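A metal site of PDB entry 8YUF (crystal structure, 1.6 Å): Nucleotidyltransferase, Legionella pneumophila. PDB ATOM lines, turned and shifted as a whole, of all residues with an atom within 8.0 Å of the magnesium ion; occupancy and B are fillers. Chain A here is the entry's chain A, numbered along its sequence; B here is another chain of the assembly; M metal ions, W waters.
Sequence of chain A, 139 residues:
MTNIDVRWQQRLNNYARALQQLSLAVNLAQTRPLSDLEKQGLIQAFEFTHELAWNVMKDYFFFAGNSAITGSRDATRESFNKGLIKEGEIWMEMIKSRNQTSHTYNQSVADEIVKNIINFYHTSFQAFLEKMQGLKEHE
OE2 of Glu 47 of chain B lies within hydrogen-bond range of OG1 of Thr 101 of chain B (2.5 Å). OE2 of Glu 47 of chain A lies within hydrogen-bond range of OG1 of Thr 101 of chain A (2.4 Å). OG1 of Thr 101 of chain B sits at hydrogen-bond distance from NE2 of Gln 44 of chain A. NE2 of Gln 44 of chain A sits at hydrogen-bond distance from OG1 of Thr 104 of chain B, 3.1 Å away. The side-chain amide nitrogen (NE2) of Gln 44 of chain B is in hydrogen-bond range of the side-chain hydroxyl (OG1) of Thr 101 of chain A, 3.1 Å away. NE2 of Gln 44 of chain B sits at hydrogen-bond distance from OG1 of Thr 104 of chain A (3.0 Å). The backbone carbonyl oxygen (O) of Thr 101 of chain A is in hydrogen-bond range of the side-chain hydroxyl (OG1) of Thr 104 of chain A. The backbone carbonyl oxygen (O) of Thr 101 of chain B sits close to the side-chain hydroxyl (OG1) of Thr 104 of chain B (3.4 Å).
Merely in contact with the magnesium ion: Thr 101 of chain A (3.9 Å) and Thr 101 of chain B (3.9 Å). Along chain A the residues within 4 Å of the magnesium ion span positions 44 to 101. The nearest printed residue that does not touch the magnesium ion is Ile 43 of chain A (5.6 Å).
The magnesium ion is bound by OE1 of Glu 47 of chain B, OE1 of Glu 47 of chain A, OE1 of Gln 44 of chain A and OE1 of Gln 44 of chain B. The magnesium ion has four donor atoms within binding distance.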
ATOM      1  N   GLN A  40       6.843   1.001  -5.664  1.00  0.00           N
ATOM      2  CA  GLN A  40       5.715   0.402  -4.985  1.00  0.00           C
ATOM      3  C   GLN A  40       5.479   1.082  -3.660  1.00  0.00           C
ATOM      4  O   GLN A  40       4.325   1.278  -3.261  1.00  0.00           O
ATOM      5  CB  GLN A  40       5.944  -1.099  -4.814  1.00  0.00           C
ATOM      6  CG  GLN A  40       6.098  -1.869  -6.115  1.00  0.00           C
ATOM      7  CD  GLN A  40       4.872  -1.812  -7.028  1.00  0.00           C
ATOM      8  OE1 GLN A  40       3.732  -1.794  -6.599  1.00  0.00           O
ATOM      9  NE2 GLN A  40       5.126  -1.811  -8.327  1.00  0.00           N
ATOM     10  N   GLY A  41       6.552   1.447  -2.961  1.00  0.00           N
ATOM     11  CA  GLY A  41       6.397   2.096  -1.658  1.00  0.00           C
ATOM     12  C   GLY A  41       5.858   3.516  -1.797  1.00  0.00           C
ATOM     13  O   GLY A  41       5.069   3.961  -0.969  1.00  0.00           O
ATOM     14  N   ILE A  43       3.750   4.359  -4.110  1.00  0.00           N
ATOM     15  CA  ILE A  43       2.322   4.186  -4.372  1.00  0.00           C
ATOM     16  C   ILE A  43       1.558   3.902  -3.076  1.00  0.00           C
ATOM     17  O   ILE A  43       0.505   4.491  -2.822  1.00  0.00           O
ATOM     18  CB  ILE A  43       2.112   3.059  -5.394  1.00  0.00           C
ATOM     19  CG1 ILE A  43       2.696   3.486  -6.714  1.00  0.00           C
ATOM     20  CG2 ILE A  43       0.654   2.641  -5.466  1.00  0.00           C
ATOM     21  CD1 ILE A  43       2.948   2.272  -7.639  1.00  0.00           C
ATOM     22  N   GLN A  44       2.098   3.019  -2.214  1.00  0.00           N
ATOM     23  CA  GLN A  44       1.495   2.758  -0.904  1.00  0.00           C
ATOM     24  C   GLN A  44       1.368   4.031  -0.078  1.00  0.00           C
ATOM     25  O   GLN A  44       0.342   4.245   0.574  1.00  0.00           O
ATOM     26  CB  GLN A  44       2.293   1.693  -0.146  1.00  0.00           C
ATOM     27  CG  GLN A  44       1.815   1.430   1.246  1.00  0.00           C
ATOM     28  CD  GLN A  44       0.451   0.780   1.309  1.00  0.00           C
ATOM     29  OE1 GLN A  44      -0.087   0.250   0.309  1.00  0.00           O
ATOM     30  NE2 GLN A  44      -0.095   0.750   2.516  1.00  0.00           N
ATOM     31  N   ALA A  45       2.415   4.874  -0.059  1.00  0.00           N
ATOM     32  CA  ALA A  45       2.304   6.165   0.656  1.00  0.00           C
ATOM     33  C   ALA A  45       1.249   7.087   0.052  1.00  0.00           C
ATOM     34  O   ALA A  45       0.512   7.792   0.768  1.00  0.00           O
ATOM     35  CB  ALA A  45       3.651   6.866   0.667  1.00  0.00           C
ATOM     36  N   PHE A  46       1.157   7.125  -1.278  1.00  0.00           N
ATOM     37  CA  PHE A  46       0.064   7.868  -1.903  1.00  0.00           C
ATOM     38  C   PHE A  46      -1.270   7.331  -1.426  1.00  0.00           C
ATOM     39  O   PHE A  46      -2.200   8.103  -1.138  1.00  0.00           O
ATOM     40  CB  PHE A  46       0.198   7.790  -3.421  1.00  0.00           C
ATOM     41  CG  PHE A  46      -1.101   7.917  -4.153  1.00  0.00           C
ATOM     42  CD1 PHE A  46      -1.768   9.115  -4.186  1.00  0.00           C
ATOM     43  CD2 PHE A  46      -1.691   6.822  -4.759  1.00  0.00           C
ATOM     44  CE1 PHE A  46      -3.027   9.241  -4.793  1.00  0.00           C
ATOM     45  CE2 PHE A  46      -2.928   6.933  -5.402  1.00  0.00           C
ATOM     46  CZ  PHE A  46      -3.614   8.118  -5.390  1.00  0.00           C
ATOM     47  N   GLU A  47      -1.399   6.017  -1.333  1.00  0.00           N
ATOM     48  CA  GLU A  47      -2.681   5.438  -0.935  1.00  0.00           C
ATOM     49  C   GLU A  47      -3.068   5.835   0.489  1.00  0.00           C
ATOM     50  O   GLU A  47      -4.235   6.174   0.759  1.00  0.00           O
ATOM     51  CB  GLU A  47      -2.692   3.924  -1.124  1.00  0.00           C
ATOM     52  CG  GLU A  47      -2.618   3.578  -2.600  1.00  0.00           C
ATOM     53  CD  GLU A  47      -2.506   2.095  -2.843  1.00  0.00           C
ATOM     54  OE1 GLU A  47      -2.326   1.347  -1.886  1.00  0.00           O
ATOM     55  OE2 GLU A  47      -2.595   1.694  -4.039  1.00  0.00           O
ATOM     56  N   PHE A  48      -2.117   5.823   1.418  1.00  0.00           N
ATOM     57  CA  PHE A  48      -2.557   6.110   2.784  1.00  0.00           C
ATOM     58  C   PHE A  48      -2.745   7.613   2.972  1.00  0.00           C
ATOM     59  O   PHE A  48      -3.561   8.044   3.809  1.00  0.00           O
ATOM     60  CB  PHE A  48      -1.663   5.507   3.880  1.00  0.00           C
ATOM     61  CG  PHE A  48      -0.201   5.872   3.880  1.00  0.00           C
ATOM     62  CD1 PHE A  48       0.212   7.180   3.953  1.00  0.00           C
ATOM     63  CD2 PHE A  48       0.760   4.865   3.974  1.00  0.00           C
ATOM     64  CE1 PHE A  48       1.566   7.505   4.014  1.00  0.00           C
ATOM     65  CE2 PHE A  48       2.069   5.156   4.058  1.00  0.00           C
ATOM     66  CZ  PHE A  48       2.486   6.492   4.110  1.00  0.00           C
ATOM     67  N   ARG A  98      -6.097   4.979  -7.370  1.00  0.00           N
ATOM     68  CA  ARG A  98      -6.399   4.058  -6.284  1.00  0.00           C
ATOM     69  C   ARG A  98      -6.953   2.770  -6.847  1.00  0.00           C
ATOM     70  O   ARG A  98      -6.645   1.689  -6.334  1.00  0.00           O
ATOM     71  CB  ARG A  98      -7.402   4.679  -5.296  1.00  0.00           C
ATOM     72  CG  ARG A  98      -6.942   5.872  -4.435  1.00  0.00           C
ATOM     73  CD  ARG A  98      -5.841   5.552  -3.448  1.00  0.00           C
ATOM     74  NE  ARG A  98      -6.205   4.506  -2.498  1.00  0.00           N
ATOM     75  CZ  ARG A  98      -6.944   4.698  -1.422  1.00  0.00           C
ATOM     76  NH1 ARG A  98      -7.444   5.901  -1.118  1.00  0.00           N
ATOM     77  NH2 ARG A  98      -7.180   3.665  -0.611  1.00  0.00           N
ATOM     78  N   THR A 101      -4.587  -0.078  -8.049  1.00  0.00           N
ATOM     79  CA  THR A 101      -3.597  -0.561  -7.098  1.00  0.00           C
ATOM     80  C   THR A 101      -3.304  -2.047  -7.293  1.00  0.00           C
ATOM     81  O   THR A 101      -2.165  -2.466  -7.173  1.00  0.00           O
ATOM     82  CB  THR A 101      -4.084  -0.285  -5.677  1.00  0.00           C
ATOM     83  OG1 THR A 101      -3.025  -0.570  -4.767  1.00  0.00           O
ATOM     84  CG2 THR A 101      -5.315  -1.137  -5.289  1.00  0.00           C
ATOM     85  N   SER A 102      -4.318  -2.838  -7.644  1.00  0.00           N
ATOM     86  CA  SER A 102      -4.120  -4.281  -7.752  1.00  0.00           C
ATOM     87  C   SER A 102      -3.244  -4.650  -8.939  1.00  0.00           C
ATOM     88  O   SER A 102      -2.736  -5.786  -8.995  1.00  0.00           O
ATOM     89  CB  SER A 102      -5.484  -4.967  -7.836  1.00  0.00           C
ATOM     90  OG  SER A 102      -6.140  -4.624  -9.041  1.00  0.00           O
ATOM     91  N   THR A 104      -0.363  -2.921 -10.084  1.00  0.00           N
ATOM     92  CA  THR A 104       0.944  -2.266 -10.128  1.00  0.00           C
ATOM     93  C   THR A 104       2.114  -3.230 -10.242  1.00  0.00           C
ATOM     94  O   THR A 104       3.247  -2.750 -10.314  1.00  0.00           O
ATOM     95  CB  THR A 104       1.105  -1.351  -8.918  1.00  0.00           C
ATOM     96  OG1 THR A 104       1.137  -2.094  -7.686  1.00  0.00           O
ATOM     97  CG2 THR A 104      -0.043  -0.345  -8.847  1.00  0.00           C
ATOM     98  N   GLN B  40       7.197  -0.112   2.733  1.00  0.00           N
ATOM     99  CA  GLN B  40       5.920   0.233   2.127  1.00  0.00           C
ATOM    100  C   GLN B  40       5.748  -0.481   0.808  1.00  0.00           C
ATOM    101  O   GLN B  40       4.660  -0.971   0.520  1.00  0.00           O
ATOM    102  CB  GLN B  40       5.798   1.740   1.958  1.00  0.00           C
ATOM    103  CG  GLN B  40       5.875   2.541   3.246  1.00  0.00           C
ATOM    104  CD  GLN B  40       4.840   2.171   4.258  1.00  0.00           C
ATOM    105  OE1 GLN B  40       3.692   1.959   3.926  1.00  0.00           O
ATOM    106  NE2 GLN B  40       5.259   2.122   5.536  1.00  0.00           N
ATOM    107  N   GLY B  41       6.814  -0.587   0.007  1.00  0.00           N
ATOM    108  CA  GLY B  41       6.738  -1.318  -1.246  1.00  0.00           C
ATOM    109  C   GLY B  41       6.526  -2.821  -1.069  1.00  0.00           C
ATOM    110  O   GLY B  41       5.813  -3.444  -1.862  1.00  0.00           O
ATOM    111  N   ILE B  43       4.868  -4.133   1.386  1.00  0.00           N
ATOM    112  CA  ILE B  43       3.460  -4.233   1.715  1.00  0.00           C
ATOM    113  C   ILE B  43       2.611  -4.155   0.459  1.00  0.00           C
ATOM    114  O   ILE B  43       1.667  -4.935   0.314  1.00  0.00           O
ATOM    115  CB  ILE B  43       3.062  -3.155   2.733  1.00  0.00           C
ATOM    116  CG1 ILE B  43       3.798  -3.419   4.033  1.00  0.00           C
ATOM    117  CG2 ILE B  43       1.591  -3.119   2.924  1.00  0.00           C
ATOM    118  CD1 ILE B  43       3.744  -2.240   5.005  1.00  0.00           C
ATOM    119  N   GLN B  44       2.891  -3.164  -0.443  1.00  0.00           N
ATOM    120  CA  GLN B  44       2.134  -3.019  -1.695  1.00  0.00           C
ATOM    121  C   GLN B  44       2.205  -4.304  -2.528  1.00  0.00           C
ATOM    122  O   GLN B  44       1.179  -4.732  -3.093  1.00  0.00           O
ATOM    123  CB  GLN B  44       2.634  -1.799  -2.494  1.00  0.00           C
ATOM    124  CG  GLN B  44       2.032  -1.666  -3.841  1.00  0.00           C
ATOM    125  CD  GLN B  44       0.551  -1.336  -3.826  1.00  0.00           C
ATOM    126  OE1 GLN B  44      -0.013  -0.934  -2.809  1.00  0.00           O
ATOM    127  NE2 GLN B  44      -0.073  -1.459  -4.989  1.00  0.00           N
ATOM    128  N   ALA B  45       3.377  -4.942  -2.569  1.00  0.00           N
ATOM    129  CA  ALA B  45       3.526  -6.200  -3.319  1.00  0.00           C
ATOM    130  C   ALA B  45       2.763  -7.346  -2.672  1.00  0.00           C
ATOM    131  O   ALA B  45       2.239  -8.226  -3.369  1.00  0.00           O
ATOM    132  CB  ALA B  45       5.000  -6.567  -3.443  1.00  0.00           C
ATOM    133  N   PHE B  46       2.744  -7.403  -1.347  1.00  0.00           N
ATOM    134  CA  PHE B  46       1.875  -8.345  -0.642  1.00  0.00           C
ATOM    135  C   PHE B  46       0.435  -8.108  -1.004  1.00  0.00           C
ATOM    136  O   PHE B  46      -0.323  -9.060  -1.250  1.00  0.00           O
ATOM    137  CB  PHE B  46       2.088  -8.252   0.869  1.00  0.00           C
ATOM    138  CG  PHE B  46       0.898  -8.641   1.677  1.00  0.00           C
ATOM    139  CD1 PHE B  46       0.507  -9.968   1.767  1.00  0.00           C
ATOM    140  CD2 PHE B  46       0.137  -7.679   2.304  1.00  0.00           C
ATOM    141  CE1 PHE B  46      -0.645 -10.331   2.509  1.00  0.00           C
ATOM    142  CE2 PHE B  46      -1.011  -8.018   3.017  1.00  0.00           C
ATOM    143  CZ  PHE B  46      -1.388  -9.343   3.106  1.00  0.00           C
ATOM    144  N   GLU B  47       0.027  -6.835  -1.103  1.00  0.00           N
ATOM    145  CA  GLU B  47      -1.368  -6.540  -1.406  1.00  0.00           C
ATOM    146  C   GLU B  47      -1.772  -6.990  -2.803  1.00  0.00           C
ATOM    147  O   GLU B  47      -2.855  -7.560  -2.996  1.00  0.00           O
ATOM    148  CB  GLU B  47      -1.675  -5.056  -1.210  1.00  0.00           C
ATOM    149  CG  GLU B  47      -1.612  -4.667   0.204  1.00  0.00           C
ATOM    150  CD  GLU B  47      -1.733  -3.173   0.451  1.00  0.00           C
ATOM    151  OE1 GLU B  47      -1.751  -2.407  -0.524  1.00  0.00           O
ATOM    152  OE2 GLU B  47      -1.839  -2.810   1.654  1.00  0.00           O
ATOM    153  N   PHE B  48      -0.917  -6.791  -3.798  1.00  0.00           N
ATOM    154  CA  PHE B  48      -1.366  -7.199  -5.130  1.00  0.00           C
ATOM    155  C   PHE B  48      -1.220  -8.707  -5.316  1.00  0.00           C
ATOM    156  O   PHE B  48      -1.959  -9.292  -6.137  1.00  0.00           O
ATOM    157  CB  PHE B  48      -0.706  -6.372  -6.254  1.00  0.00           C
ATOM    158  CG  PHE B  48       0.803  -6.415  -6.401  1.00  0.00           C
ATOM    159  CD1 PHE B  48       1.501  -7.593  -6.455  1.00  0.00           C
ATOM    160  CD2 PHE B  48       1.486  -5.226  -6.527  1.00  0.00           C
ATOM    161  CE1 PHE B  48       2.884  -7.605  -6.643  1.00  0.00           C
ATOM    162  CE2 PHE B  48       2.877  -5.202  -6.789  1.00  0.00           C
ATOM    163  CZ  PHE B  48       3.586  -6.414  -6.830  1.00  0.00           C
ATOM    164  N   ARG B  98      -4.327  -6.815   5.255  1.00  0.00           N
ATOM    165  CA  ARG B  98      -4.924  -5.993   4.200  1.00  0.00           C
ATOM    166  C   ARG B  98      -5.742  -4.845   4.790  1.00  0.00           C
ATOM    167  O   ARG B  98      -5.684  -3.729   4.281  1.00  0.00           O
ATOM    168  CB  ARG B  98      -5.816  -6.834   3.286  1.00  0.00           C
ATOM    169  CG  ARG B  98      -5.139  -7.884   2.410  1.00  0.00           C
ATOM    170  CD  ARG B  98      -4.233  -7.337   1.339  1.00  0.00           C
ATOM    171  NE  ARG B  98      -4.885  -6.427   0.402  1.00  0.00           N
ATOM    172  CZ  ARG B  98      -5.625  -6.817  -0.634  1.00  0.00           C
ATOM    173  NH1 ARG B  98      -5.791  -8.105  -0.919  1.00  0.00           N
ATOM    174  NH2 ARG B  98      -6.223  -5.887  -1.396  1.00  0.00           N
ATOM    175  N   THR B 101      -3.965  -1.528   5.866  1.00  0.00           N
ATOM    176  CA  THR B 101      -3.176  -0.865   4.842  1.00  0.00           C
ATOM    177  C   THR B 101      -3.172   0.642   5.036  1.00  0.00           C
ATOM    178  O   THR B 101      -2.148   1.287   4.801  1.00  0.00           O
ATOM    179  CB  THR B 101      -3.716  -1.237   3.456  1.00  0.00           C
ATOM    180  OG1 THR B 101      -2.849  -0.706   2.443  1.00  0.00           O
ATOM    181  CG2 THR B 101      -5.115  -0.698   3.212  1.00  0.00           C
ATOM    182  N   SER B 102      -4.302   1.207   5.464  1.00  0.00           N
ATOM    183  CA  SER B 102      -4.416   2.659   5.544  1.00  0.00           C
ATOM    184  C   SER B 102      -3.587   3.235   6.685  1.00  0.00           C
ATOM    185  O   SER B 102      -3.379   4.461   6.733  1.00  0.00           O
ATOM    186  CB  SER B 102      -5.893   3.055   5.684  1.00  0.00           C
ATOM    187  OG  SER B 102      -6.396   2.712   6.948  1.00  0.00           O
ATOM    188  N   THR B 104      -0.340   2.216   7.583  1.00  0.00           N
ATOM    189  CA  THR B 104       1.053   1.836   7.552  1.00  0.00           C
ATOM    190  C   THR B 104       2.007   3.017   7.617  1.00  0.00           C
ATOM    191  O   THR B 104       3.233   2.804   7.593  1.00  0.00           O
ATOM    192  CB  THR B 104       1.335   0.964   6.330  1.00  0.00           C
ATOM    193  OG1 THR B 104       1.232   1.718   5.125  1.00  0.00           O
ATOM    194  CG2 THR B 104       0.415  -0.253   6.305  1.00  0.00           C
HETATM  195 MG    MG M   1      -1.472  -0.514  -1.216  1.00  0.00          MG
HETATM  196  O   HOH W   1      -3.437   0.774   0.406  1.00  0.00           O
HETATM  197  O   HOH W   2      -3.283  -2.504  -2.736  1.00  0.00           O
